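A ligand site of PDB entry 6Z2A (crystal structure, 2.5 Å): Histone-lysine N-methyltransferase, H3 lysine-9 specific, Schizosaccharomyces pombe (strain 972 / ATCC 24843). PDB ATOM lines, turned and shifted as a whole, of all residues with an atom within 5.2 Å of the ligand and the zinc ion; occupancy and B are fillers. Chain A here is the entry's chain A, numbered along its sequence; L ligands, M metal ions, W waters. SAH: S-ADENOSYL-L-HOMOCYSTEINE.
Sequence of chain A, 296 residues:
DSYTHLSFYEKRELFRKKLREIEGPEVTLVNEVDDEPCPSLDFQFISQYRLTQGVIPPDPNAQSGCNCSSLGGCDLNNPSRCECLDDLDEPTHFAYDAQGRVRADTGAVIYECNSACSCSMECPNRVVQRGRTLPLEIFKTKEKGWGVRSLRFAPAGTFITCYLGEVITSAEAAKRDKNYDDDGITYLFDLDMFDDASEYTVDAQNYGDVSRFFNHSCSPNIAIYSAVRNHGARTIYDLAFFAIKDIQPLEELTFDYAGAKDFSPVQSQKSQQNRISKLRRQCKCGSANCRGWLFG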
ATOM      1  N   GLU A 143      -7.144  20.669   9.198  1.00  0.00           N
ATOM      2  CA  GLU A 143      -7.922  20.242  10.395  1.00  0.00           C
ATOM      3  C   GLU A 143      -7.045  19.505  11.412  1.00  0.00           C
ATOM      4  O   GLU A 143      -7.595  19.164  12.478  1.00  0.00           O
ATOM      5  CB  GLU A 143      -9.079  19.327   9.989  1.00  0.00           C
ATOM      6  CG  GLU A 143     -10.087  19.991   9.073  1.00  0.00           C
ATOM      7  CD  GLU A 143     -11.273  19.118   8.675  1.00  0.00           C
ATOM      8  OE1 GLU A 143     -11.634  18.249   9.472  1.00  0.00           O
ATOM      9  OE2 GLU A 143     -11.840  19.325   7.576  1.00  0.00           O
ATOM     10  N   LYS A 144      -5.756  19.276  11.144  1.00  0.00           N
ATOM     11  CA  LYS A 144      -4.905  18.357  11.939  1.00  0.00           C
ATOM     12  C   LYS A 144      -3.671  19.077  12.486  1.00  0.00           C
ATOM     13  O   LYS A 144      -2.753  18.348  12.930  1.00  0.00           O
ATOM     14  CB  LYS A 144      -4.475  17.169  11.084  1.00  0.00           C
ATOM     15  CG  LYS A 144      -5.612  16.413  10.416  1.00  0.00           C
ATOM     16  CD  LYS A 144      -5.121  15.350   9.464  1.00  0.00           C
ATOM     17  CE  LYS A 144      -4.217  15.939   8.396  1.00  0.00           C
ATOM     18  NZ  LYS A 144      -4.148  15.078   7.192  1.00  0.00           N
ATOM     19  N   GLY A 145      -3.661  20.406  12.498  1.00  0.00           N
ATOM     20  CA  GLY A 145      -2.488  21.210  12.904  1.00  0.00           C
ATOM     21  C   GLY A 145      -1.412  21.141  11.850  1.00  0.00           C
ATOM     22  O   GLY A 145      -1.762  21.093  10.664  1.00  0.00           O
ATOM     23  N   TRP A 146      -0.149  21.109  12.254  1.00  0.00           N
ATOM     24  CA  TRP A 146       1.016  21.069  11.324  1.00  0.00           C
ATOM     25  C   TRP A 146       1.169  19.671  10.730  1.00  0.00           C
ATOM     26  O   TRP A 146       0.645  18.685  11.290  1.00  0.00           O
ATOM     27  CB  TRP A 146       2.296  21.536  12.012  1.00  0.00           C
ATOM     28  CG  TRP A 146       2.222  22.966  12.458  1.00  0.00           C
ATOM     29  CD1 TRP A 146       1.982  23.416  13.717  1.00  0.00           C
ATOM     30  CD2 TRP A 146       2.410  24.129  11.645  1.00  0.00           C
ATOM     31  NE1 TRP A 146       1.991  24.783  13.748  1.00  0.00           N
ATOM     32  CE2 TRP A 146       2.249  25.252  12.480  1.00  0.00           C
ATOM     33  CE3 TRP A 146       2.687  24.343  10.285  1.00  0.00           C
ATOM     34  CZ2 TRP A 146       2.364  26.560  12.015  1.00  0.00           C
ATOM     35  CZ3 TRP A 146       2.801  25.639   9.827  1.00  0.00           C
ATOM     36  CH2 TRP A 146       2.644  26.730  10.679  1.00  0.00           C
ATOM     37  N   GLY A 147       1.848  19.592   9.595  1.00  0.00           N
ATOM     38  CA  GLY A 147       2.011  18.370   8.815  1.00  0.00           C
ATOM     39  C   GLY A 147       3.278  18.476   8.012  1.00  0.00           C
ATOM     40  O   GLY A 147       3.925  19.534   8.072  1.00  0.00           O
ATOM     41  N   GLY A 184      -0.497  20.446  19.083  1.00  0.00           N
ATOM     42  CA  GLY A 184       0.958  20.248  19.021  1.00  0.00           C
ATOM     43  C   GLY A 184       1.453  19.383  20.173  1.00  0.00           C
ATOM     44  O   GLY A 184       2.651  19.468  20.512  1.00  0.00           O
ATOM     45  N   ILE A 185       0.586  18.558  20.758  1.00  0.00           N
ATOM     46  CA  ILE A 185       1.009  17.566  21.778  1.00  0.00           C
ATOM     47  C   ILE A 185       1.238  16.238  21.055  1.00  0.00           C
ATOM     48  O   ILE A 185       0.249  15.611  20.613  1.00  0.00           O
ATOM     49  CB  ILE A 185       0.014  17.449  22.938  1.00  0.00           C
ATOM     50  CG1 ILE A 185      -0.342  18.837  23.485  1.00  0.00           C
ATOM     51  CG2 ILE A 185       0.572  16.542  24.008  1.00  0.00           C
ATOM     52  CD1 ILE A 185      -0.805  18.847  24.916  1.00  0.00           C
ATOM     53  N   THR A 186       2.500  15.816  20.928  1.00  0.00           N
ATOM     54  CA  THR A 186       2.867  14.467  20.431  1.00  0.00           C
ATOM     55  C   THR A 186       2.442  13.444  21.477  1.00  0.00           C
ATOM     56  O   THR A 186       2.338  13.806  22.659  1.00  0.00           O
ATOM     57  CB  THR A 186       4.371  14.288  20.182  1.00  0.00           C
ATOM     58  OG1 THR A 186       5.028  14.152  21.446  1.00  0.00           O
ATOM     59  CG2 THR A 186       4.988  15.411  19.377  1.00  0.00           C
ATOM     60  N   TYR A 187       2.234  12.195  21.071  1.00  0.00           N
ATOM     61  CA  TYR A 187       2.117  11.062  22.020  1.00  0.00           C
ATOM     62  C   TYR A 187       3.349  10.170  21.878  1.00  0.00           C
ATOM     63  O   TYR A 187       4.224  10.406  21.017  1.00  0.00           O
ATOM     64  CB  TYR A 187       0.757  10.384  21.861  1.00  0.00           C
ATOM     65  CG  TYR A 187      -0.404  11.262  22.256  1.00  0.00           C
ATOM     66  CD1 TYR A 187      -0.500  11.787  23.537  1.00  0.00           C
ATOM     67  CD2 TYR A 187      -1.407  11.590  21.343  1.00  0.00           C
ATOM     68  CE1 TYR A 187      -1.567  12.592  23.913  1.00  0.00           C
ATOM     69  CE2 TYR A 187      -2.471  12.394  21.704  1.00  0.00           C
ATOM     70  CZ  TYR A 187      -2.552  12.907  22.996  1.00  0.00           C
ATOM     71  OH  TYR A 187      -3.607  13.695  23.373  1.00  0.00           O
ATOM     72  N   ARG A 212       8.319  14.313  13.659  1.00  0.00           N
ATOM     73  CA  ARG A 212       7.541  14.713  14.793  1.00  0.00           C
ATOM     74  C   ARG A 212       6.254  15.390  14.354  1.00  0.00           C
ATOM     75  O   ARG A 212       5.307  15.360  15.037  1.00  0.00           O
ATOM     76  CB  ARG A 212       8.354  15.635  15.682  1.00  0.00           C
ATOM     77  CG  ARG A 212       7.644  16.232  16.858  1.00  0.00           C
ATOM     78  CD  ARG A 212       7.352  17.675  16.617  1.00  0.00           C
ATOM     79  NE  ARG A 212       6.710  18.332  17.727  1.00  0.00           N
ATOM     80  CZ  ARG A 212       5.405  18.381  17.910  1.00  0.00           C
ATOM     81  NH1 ARG A 212       4.605  17.769  17.100  1.00  0.00           N
ATOM     82  NH2 ARG A 212       4.921  19.010  18.921  1.00  0.00           N
ATOM     83  N   PHE A 213       6.256  15.913  13.142  1.00  0.00           N
ATOM     84  CA  PHE A 213       5.105  16.618  12.518  1.00  0.00           C
ATOM     85  C   PHE A 213       4.334  15.724  11.534  1.00  0.00           C
ATOM     86  O   PHE A 213       3.356  16.228  10.979  1.00  0.00           O
ATOM     87  CB  PHE A 213       5.592  17.890  11.832  1.00  0.00           C
ATOM     88  CG  PHE A 213       6.257  18.843  12.785  1.00  0.00           C
ATOM     89  CD1 PHE A 213       5.506  19.548  13.714  1.00  0.00           C
ATOM     90  CD2 PHE A 213       7.626  19.017  12.764  1.00  0.00           C
ATOM     91  CE1 PHE A 213       6.115  20.430  14.600  1.00  0.00           C
ATOM     92  CE2 PHE A 213       8.230  19.895  13.642  1.00  0.00           C
ATOM     93  CZ  PHE A 213       7.486  20.603  14.564  1.00  0.00           C
ATOM     94  N   PHE A 214       4.762  14.475  11.297  1.00  0.00           N
ATOM     95  CA  PHE A 214       3.974  13.507  10.471  1.00  0.00           C
ATOM     96  C   PHE A 214       2.636  13.229  11.166  1.00  0.00           C
ATOM     97  O   PHE A 214       2.614  12.998  12.396  1.00  0.00           O
ATOM     98  CB  PHE A 214       4.699  12.183  10.270  1.00  0.00           C
ATOM     99  CG  PHE A 214       5.951  12.228   9.447  1.00  0.00           C
ATOM    100  CD1 PHE A 214       6.278  13.331   8.670  1.00  0.00           C
ATOM    101  CD2 PHE A 214       6.798  11.130   9.408  1.00  0.00           C
ATOM    102  CE1 PHE A 214       7.428  13.340   7.907  1.00  0.00           C
ATOM    103  CE2 PHE A 214       7.959  11.159   8.652  1.00  0.00           C
ATOM    104  CZ  PHE A 214       8.270  12.269   7.908  1.00  0.00           C
ATOM    105  N   ASN A 215       1.550  13.219  10.395  1.00  0.00           N
ATOM    106  CA  ASN A 215       0.173  12.999  10.910  1.00  0.00           C
ATOM    107  C   ASN A 215      -0.236  11.543  10.673  1.00  0.00           C
ATOM    108  O   ASN A 215       0.431  10.827   9.898  1.00  0.00           O
ATOM    109  CB  ASN A 215      -0.818  13.997  10.307  1.00  0.00           C
ATOM    110  CG  ASN A 215      -0.673  15.387  10.898  1.00  0.00           C
ATOM    111  OD1 ASN A 215      -0.715  15.552  12.113  1.00  0.00           O
ATOM    112  ND2 ASN A 215      -0.490  16.384  10.050  1.00  0.00           N
ATOM    113  N   HIS A 216      -1.311  11.123  11.346  1.00  0.00           N
ATOM    114  CA  HIS A 216      -1.871   9.760  11.206  1.00  0.00           C
ATOM    115  C   HIS A 216      -2.813   9.714  10.005  1.00  0.00           C
ATOM    116  O   HIS A 216      -3.637  10.654   9.842  1.00  0.00           O
ATOM    117  CB  HIS A 216      -2.622   9.299  12.458  1.00  0.00           C
ATOM    118  CG  HIS A 216      -3.565   8.179  12.163  1.00  0.00           C
ATOM    119  ND1 HIS A 216      -3.142   6.908  11.876  1.00  0.00           N
ATOM    120  CD2 HIS A 216      -4.902   8.166  12.058  1.00  0.00           C
ATOM    121  CE1 HIS A 216      -4.178   6.146  11.636  1.00  0.00           C
ATOM    122  NE2 HIS A 216      -5.285   6.897  11.737  1.00  0.00           N
ATOM    123  N   SER A 217      -2.731   8.633   9.236  1.00  0.00           N
ATOM    124  CA  SER A 217      -3.759   8.279   8.240  1.00  0.00           C
ATOM    125  C   SER A 217      -4.147   6.809   8.421  1.00  0.00           C
ATOM    126  O   SER A 217      -3.266   5.983   8.693  1.00  0.00           O
ATOM    127  CB  SER A 217      -3.323   8.545   6.841  1.00  0.00           C
ATOM    128  OG  SER A 217      -4.368   8.241   5.934  1.00  0.00           O
ATOM    129  N   CYS A 218      -5.445   6.528   8.285  1.00  0.00           N
ATOM    130  CA  CYS A 218      -5.975   5.148   8.229  1.00  0.00           C
ATOM    131  C   CYS A 218      -5.620   4.531   6.872  1.00  0.00           C
ATOM    132  O   CYS A 218      -5.781   3.314   6.734  1.00  0.00           O
ATOM    133  CB  CYS A 218      -7.485   5.139   8.459  1.00  0.00           C
ATOM    134  SG  CYS A 218      -7.949   5.958   9.955  1.00  0.00           S
ATOM    135  N   TYR A 257      -0.587   5.352  12.949  1.00  0.00           N
ATOM    136  CA  TYR A 257      -0.107   5.419  14.345  1.00  0.00           C
ATOM    137  C   TYR A 257      -0.426   4.121  15.083  1.00  0.00           C
ATOM    138  O   TYR A 257       0.327   3.806  15.991  1.00  0.00           O
ATOM    139  CB  TYR A 257      -0.788   6.578  15.074  1.00  0.00           C
ATOM    140  CG  TYR A 257      -0.330   8.003  14.848  1.00  0.00           C
ATOM    141  CD1 TYR A 257       0.502   8.354  13.804  1.00  0.00           C
ATOM    142  CD2 TYR A 257      -0.796   9.007  15.685  1.00  0.00           C
ATOM    143  CE1 TYR A 257       0.877   9.669  13.615  1.00  0.00           C
ATOM    144  CE2 TYR A 257      -0.426  10.330  15.495  1.00  0.00           C
ATOM    145  CZ  TYR A 257       0.410  10.661  14.460  1.00  0.00           C
ATOM    146  OH  TYR A 257       0.792  11.955  14.266  1.00  0.00           O
ATOM    147  N   LYS A 261       2.654   4.799  17.511  1.00  0.00           N
ATOM    148  CA  LYS A 261       2.490   6.047  18.211  1.00  0.00           C
ATOM    149  C   LYS A 261       1.136   6.010  18.885  1.00  0.00           C
ATOM    150  O   LYS A 261       0.191   5.601  18.317  1.00  0.00           O
ATOM    151  CB  LYS A 261       2.659   7.235  17.237  1.00  0.00           C
ATOM    152  CG  LYS A 261       2.544   8.624  17.851  1.00  0.00           C
ATOM    153  CD  LYS A 261       3.105   9.738  16.983  1.00  0.00           C
ATOM    154  CE  LYS A 261       2.858  11.091  17.624  1.00  0.00           C
ATOM    155  NZ  LYS A 261       3.613  12.225  17.095  1.00  0.00           N
ATOM    156  N   ARG A 281     -11.176  13.892  20.259  1.00  0.00           N
ATOM    157  CA  ARG A 281     -11.199  14.473  18.884  1.00  0.00           C
ATOM    158  C   ARG A 281     -10.914  13.358  17.857  1.00  0.00           C
ATOM    159  O   ARG A 281      -9.908  12.645  17.997  1.00  0.00           O
ATOM    160  CB  ARG A 281     -10.221  15.652  18.831  1.00  0.00           C
ATOM    161  CG  ARG A 281      -9.397  15.821  17.567  1.00  0.00           C
ATOM    162  CD  ARG A 281      -8.268  16.789  17.881  1.00  0.00           C
ATOM    163  NE  ARG A 281      -7.295  16.988  16.806  1.00  0.00           N
ATOM    164  CZ  ARG A 281      -6.894  18.169  16.321  1.00  0.00           C
ATOM    165  NH1 ARG A 281      -7.384  19.312  16.791  1.00  0.00           N
ATOM    166  NH2 ARG A 281      -6.002  18.208  15.351  1.00  0.00           N
ATOM    167  N   GLN A 282     -11.790  13.237  16.855  1.00  0.00           N
ATOM    168  CA  GLN A 282     -11.844  12.078  15.914  1.00  0.00           C
ATOM    169  C   GLN A 282     -10.720  12.176  14.879  1.00  0.00           C
ATOM    170  O   GLN A 282      -9.981  13.193  14.889  1.00  0.00           O
ATOM    171  CB  GLN A 282     -13.202  12.028  15.209  1.00  0.00           C
ATOM    172  CG  GLN A 282     -14.346  11.647  16.142  1.00  0.00           C
ATOM    173  CD  GLN A 282     -15.540  11.153  15.374  1.00  0.00           C
ATOM    174  OE1 GLN A 282     -16.238  11.928  14.721  1.00  0.00           O
ATOM    175  NE2 GLN A 282     -15.781   9.849  15.430  1.00  0.00           N
ATOM    176  N   CYS A 283     -10.635  11.168  14.013  1.00  0.00           N
ATOM    177  CA  CYS A 283      -9.681  11.090  12.872  1.00  0.00           C
ATOM    178  C   CYS A 283     -10.199  11.964  11.716  1.00  0.00           C
ATOM    179  O   CYS A 283     -11.384  11.837  11.367  1.00  0.00           O
ATOM    180  CB  CYS A 283      -9.484   9.657  12.414  1.00  0.00           C
ATOM    181  SG  CYS A 283      -8.128   9.539  11.313  1.00  0.00           S
ATOM    182  N   LYS A 284      -9.324  12.799  11.161  1.00  0.00           N
ATOM    183  CA  LYS A 284      -9.618  13.730  10.039  1.00  0.00           C
ATOM    184  C   LYS A 284      -8.750  13.381   8.843  1.00  0.00           C
ATOM    185  O   LYS A 284      -8.462  14.290   8.071  1.00  0.00           O
ATOM    186  CB  LYS A 284      -9.339  15.174  10.459  1.00  0.00           C
ATOM    187  CG  LYS A 284     -10.005  15.612  11.763  1.00  0.00           C
ATOM    188  CD  LYS A 284     -11.509  15.452  11.745  1.00  0.00           C
ATOM    189  CE  LYS A 284     -12.157  15.957  13.012  1.00  0.00           C
ATOM    190  NZ  LYS A 284     -13.588  16.263  12.772  1.00  0.00           N
ATOM    191  N   CYS A 285      -8.348  12.112   8.675  1.00  0.00           N
ATOM    192  CA  CYS A 285      -7.479  11.665   7.548  1.00  0.00           C
ATOM    193  C   CYS A 285      -8.283  11.684   6.235  1.00  0.00           C
ATOM    194  O   CYS A 285      -7.678  11.941   5.180  1.00  0.00           O
ATOM    195  CB  CYS A 285      -6.859  10.308   7.871  1.00  0.00           C
ATOM    196  SG  CYS A 285      -7.868   8.899   7.559  1.00  0.00           S
ATOM    197  N   GLY A 286      -9.597  11.434   6.317  1.00  0.00           N
ATOM    198  CA  GLY A 286     -10.542  11.604   5.205  1.00  0.00           C
ATOM    199  C   GLY A 286     -10.549  10.415   4.265  1.00  0.00           C
ATOM    200  O   GLY A 286     -11.250  10.505   3.240  1.00  0.00           O
ATOM    201  N   CYS A 290     -11.455   5.063   6.539  1.00  0.00           N
ATOM    202  CA  CYS A 290     -11.157   5.698   7.846  1.00  0.00           C
ATOM    203  C   CYS A 290     -11.873   4.940   8.969  1.00  0.00           C
ATOM    204  O   CYS A 290     -13.084   4.644   8.838  1.00  0.00           O
ATOM    205  CB  CYS A 290     -11.526   7.177   7.886  1.00  0.00           C
ATOM    206  SG  CYS A 290     -11.112   7.948   9.437  1.00  0.00           S
ATOM    207  N   ARG A 291     -11.136   4.650  10.045  1.00  0.00           N
ATOM    208  CA  ARG A 291     -11.565   3.807  11.188  1.00  0.00           C
ATOM    209  C   ARG A 291     -12.234   4.672  12.263  1.00  0.00           C
ATOM    210  O   ARG A 291     -12.752   4.110  13.237  1.00  0.00           O
ATOM    211  CB  ARG A 291     -10.363   3.070  11.770  1.00  0.00           C
ATOM    212  CG  ARG A 291      -9.506   2.325  10.742  1.00  0.00           C
ATOM    213  CD  ARG A 291     -10.134   1.062  10.167  1.00  0.00           C
ATOM    214  NE  ARG A 291     -10.072  -0.090  11.076  1.00  0.00           N
ATOM    215  CZ  ARG A 291      -9.019  -0.913  11.236  1.00  0.00           C
ATOM    216  NH1 ARG A 291      -7.918  -0.775  10.510  1.00  0.00           N
ATOM    217  NH2 ARG A 291      -9.094  -1.909  12.105  1.00  0.00           N
ATOM    218  N   GLY A 292     -12.174   6.001  12.124  1.00  0.00           N
ATOM    219  CA  GLY A 292     -12.787   6.956  13.059  1.00  0.00           C
ATOM    220  C   GLY A 292     -12.086   6.958  14.401  1.00  0.00           C
ATOM    221  O   GLY A 292     -12.761   7.276  15.410  1.00  0.00           O
ATOM    222  N   PHE A 295      -8.578  10.749  19.041  1.00  0.00           N
ATOM    223  CA  PHE A 295      -7.332  11.334  19.604  1.00  0.00           C
ATOM    224  C   PHE A 295      -7.606  11.902  21.002  1.00  0.00           C
ATOM    225  O   PHE A 295      -8.734  12.384  21.272  1.00  0.00           O
ATOM    226  CB  PHE A 295      -6.696  12.327  18.637  1.00  0.00           C
ATOM    227  CG  PHE A 295      -6.086  11.669  17.416  1.00  0.00           C
ATOM    228  CD1 PHE A 295      -6.846  11.381  16.302  1.00  0.00           C
ATOM    229  CD2 PHE A 295      -4.745  11.304  17.404  1.00  0.00           C
ATOM    230  CE1 PHE A 295      -6.278  10.770  15.186  1.00  0.00           C
ATOM    231  CE2 PHE A 295      -4.183  10.701  16.287  1.00  0.00           C
ATOM    232  CZ  PHE A 295      -4.949  10.434  15.179  1.00  0.00           C
HETATM  233  N   SAH L   1      -0.260  17.907  13.881  1.00  0.00           N
HETATM  234  CA  SAH L   1       0.835  17.870  14.884  1.00  0.00           C
HETATM  235  CB  SAH L   1       2.005  17.020  14.374  1.00  0.00           C
HETATM  236  CG  SAH L   1       1.892  15.551  14.720  1.00  0.00           C
HETATM  237  SD  SAH L   1       1.923  15.276  16.509  1.00  0.00           S
HETATM  238  C   SAH L   1       1.292  19.296  15.186  1.00  0.00           C
HETATM  239  O   SAH L   1       0.552  20.218  14.834  1.00  0.00           O
HETATM  240  OXT SAH L   1       2.360  19.486  15.774  1.00  0.00           O
HETATM  241  C5' SAH L   1       0.459  14.231  16.734  1.00  0.00           C
HETATM  242  C4' SAH L   1      -0.851  14.961  16.874  1.00  0.00           C
HETATM  243  O4' SAH L   1      -1.359  15.324  15.567  1.00  0.00           O
HETATM  244  C3' SAH L   1      -1.962  14.122  17.491  1.00  0.00           C
HETATM  245  O3' SAH L   1      -1.876  14.135  18.909  1.00  0.00           O
HETATM  246  C2' SAH L   1      -3.219  14.844  16.967  1.00  0.00           C
HETATM  247  O2' SAH L   1      -3.581  15.938  17.778  1.00  0.00           O
HETATM  248  C1' SAH L   1      -2.771  15.302  15.582  1.00  0.00           C
HETATM  249  N9  SAH L   1      -3.209  14.423  14.505  1.00  0.00           N
HETATM  250  C8  SAH L   1      -2.428  13.572  13.773  1.00  0.00           C
HETATM  251  N7  SAH L   1      -3.083  12.899  12.864  1.00  0.00           N
HETATM  252  C5  SAH L   1      -4.401  13.310  13.019  1.00  0.00           C
HETATM  253  C6  SAH L   1      -5.582  12.960  12.346  1.00  0.00           C
HETATM  254  N6  SAH L   1      -5.632  12.064  11.371  1.00  0.00           N
HETATM  255  N1  SAH L   1      -6.726  13.547  12.751  1.00  0.00           N
HETATM  256  C2  SAH L   1      -6.660  14.443  13.742  1.00  0.00           C
HETATM  257  N3  SAH L   1      -5.603  14.871  14.438  1.00  0.00           N
HETATM  258  C4  SAH L   1      -4.482  14.256  14.024  1.00  0.00           C
HETATM  259 ZN    ZN M   1      -8.790   8.139   9.569  1.00  0.00          ZN
HETATM  260  O   HOH W   1       3.166  21.961  17.232  1.00  0.00           O
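N6 of the ligand sits close to SG of Cys 283 (3.6 Å). A nitrogen (N) of the ligand is in hydrogen-bond range of the backbone carbonyl oxygen of Lys 144. The backbone NH of Trp 146 lies within hydrogen-bond range of an oxygen (O) of the ligand (2.8 Å). The backbone carbonyl oxygen of Trp 146 is in hydrogen-bond range of a nitrogen (N) of the ligand (2.9 Å). The backbone NH of His 216 lies within hydrogen-bond range of a nitrogen (N7) of the ligand. O of His 216 is in hydrogen-bond range of N6 of the ligand, at 2.9 Å. OD1 of Asn 215 sits at hydrogen-bond distance from N of the ligand (3.0 Å). The backbone carbonyl oxygen of Ile 185 sits at hydrogen-bond distance from an oxygen (O3') of the ligand. The guanidinium group of Arg 212 is in salt-bridge range of an oxygen (OXT) of the ligand (3.1 Å). The backbone NH (N) of Lys 284 lies within hydrogen-bond range of a nitrogen (N1) of the ligand, at 3.1 Å. N3 of the ligand lies within hydrogen-bond range of NH2 of Arg 281 (3.5 Å). The side-chain amino group (NZ) of Lys 261 lies close to a sulfur (SD) of the ligand (3.5 Å).
The backbone NH (N) of Gly 292 sits close to the side-chain sulfur (SG) of Cys 290 (3.5 Å). The backbone NH (N) of Cys 218 sits at hydrogen-bond distance from a ring nitrogen (NE2) of His 216, at 3.5 Å. The side-chain sulfur (SG) of Cys 218 lies close to the backbone NH (N) of Arg 291 (3.4 Å). The backbone carbonyl oxygen (O) of Trp 146 lies within hydrogen-bond range of the side-chain amide nitrogen (ND2) of Asn 215. N of Tyr 257 lies within hydrogen-bond range of ND1 of His 216, at 3.2 Å. The side-chain hydroxyl (OH) of Tyr 257 lies within hydrogen-bond range of the backbone carbonyl oxygen (O) of Phe 214, 2.8 Å away. The backbone carbonyl oxygen of Arg 281 sits at hydrogen-bond distance from the backbone NH of Phe 295. NH2 of Arg 281 lies within hydrogen-bond range of O of Glu 143, 3.4 Å away.
C of Gly 145 touches O of the ligand, at 3.7 Å. Gly 184 touches the ligand. CE2 of Tyr 187 touches O3' of the ligand, 3.3 Å away. CA of Phe 213 touches CB of the ligand, at 3.6 Å. O of Phe 214 touches CG of the ligand, at 3.5 Å. OH of Tyr 257 touches C5' of the ligand, 3.4 Å away. Gln 282 touches the ligand (O to C2, 3.7 Å). CZ of Phe 295 touches C5 of the ligand (3.6 Å). Hydrophobic or aromatic side chains that line the ligand: Trp 146, Tyr 187, Phe 213, His 216 and Phe 295. Within 4 Å of the ligand: Lys 144, Gly 145, Trp 146, Gly 184, Ile 185, Tyr 187, Arg 212, Phe 213, Phe 214, Asn 215, His 216, Tyr 257, Lys 261, Arg 281, Gln 282, Cys 283, Lys 284, Cys 285 and Phe 295. Along chain A the residues within 4 Å of the ligand span positions 144 to 295.
The zinc ion is bound by SG of Cys 283 (2.3 Å), SG of Cys 290 (2.3 Å), SG of Cys 285 (2.3 Å) and SG of Cys 218 (2.4 Å).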
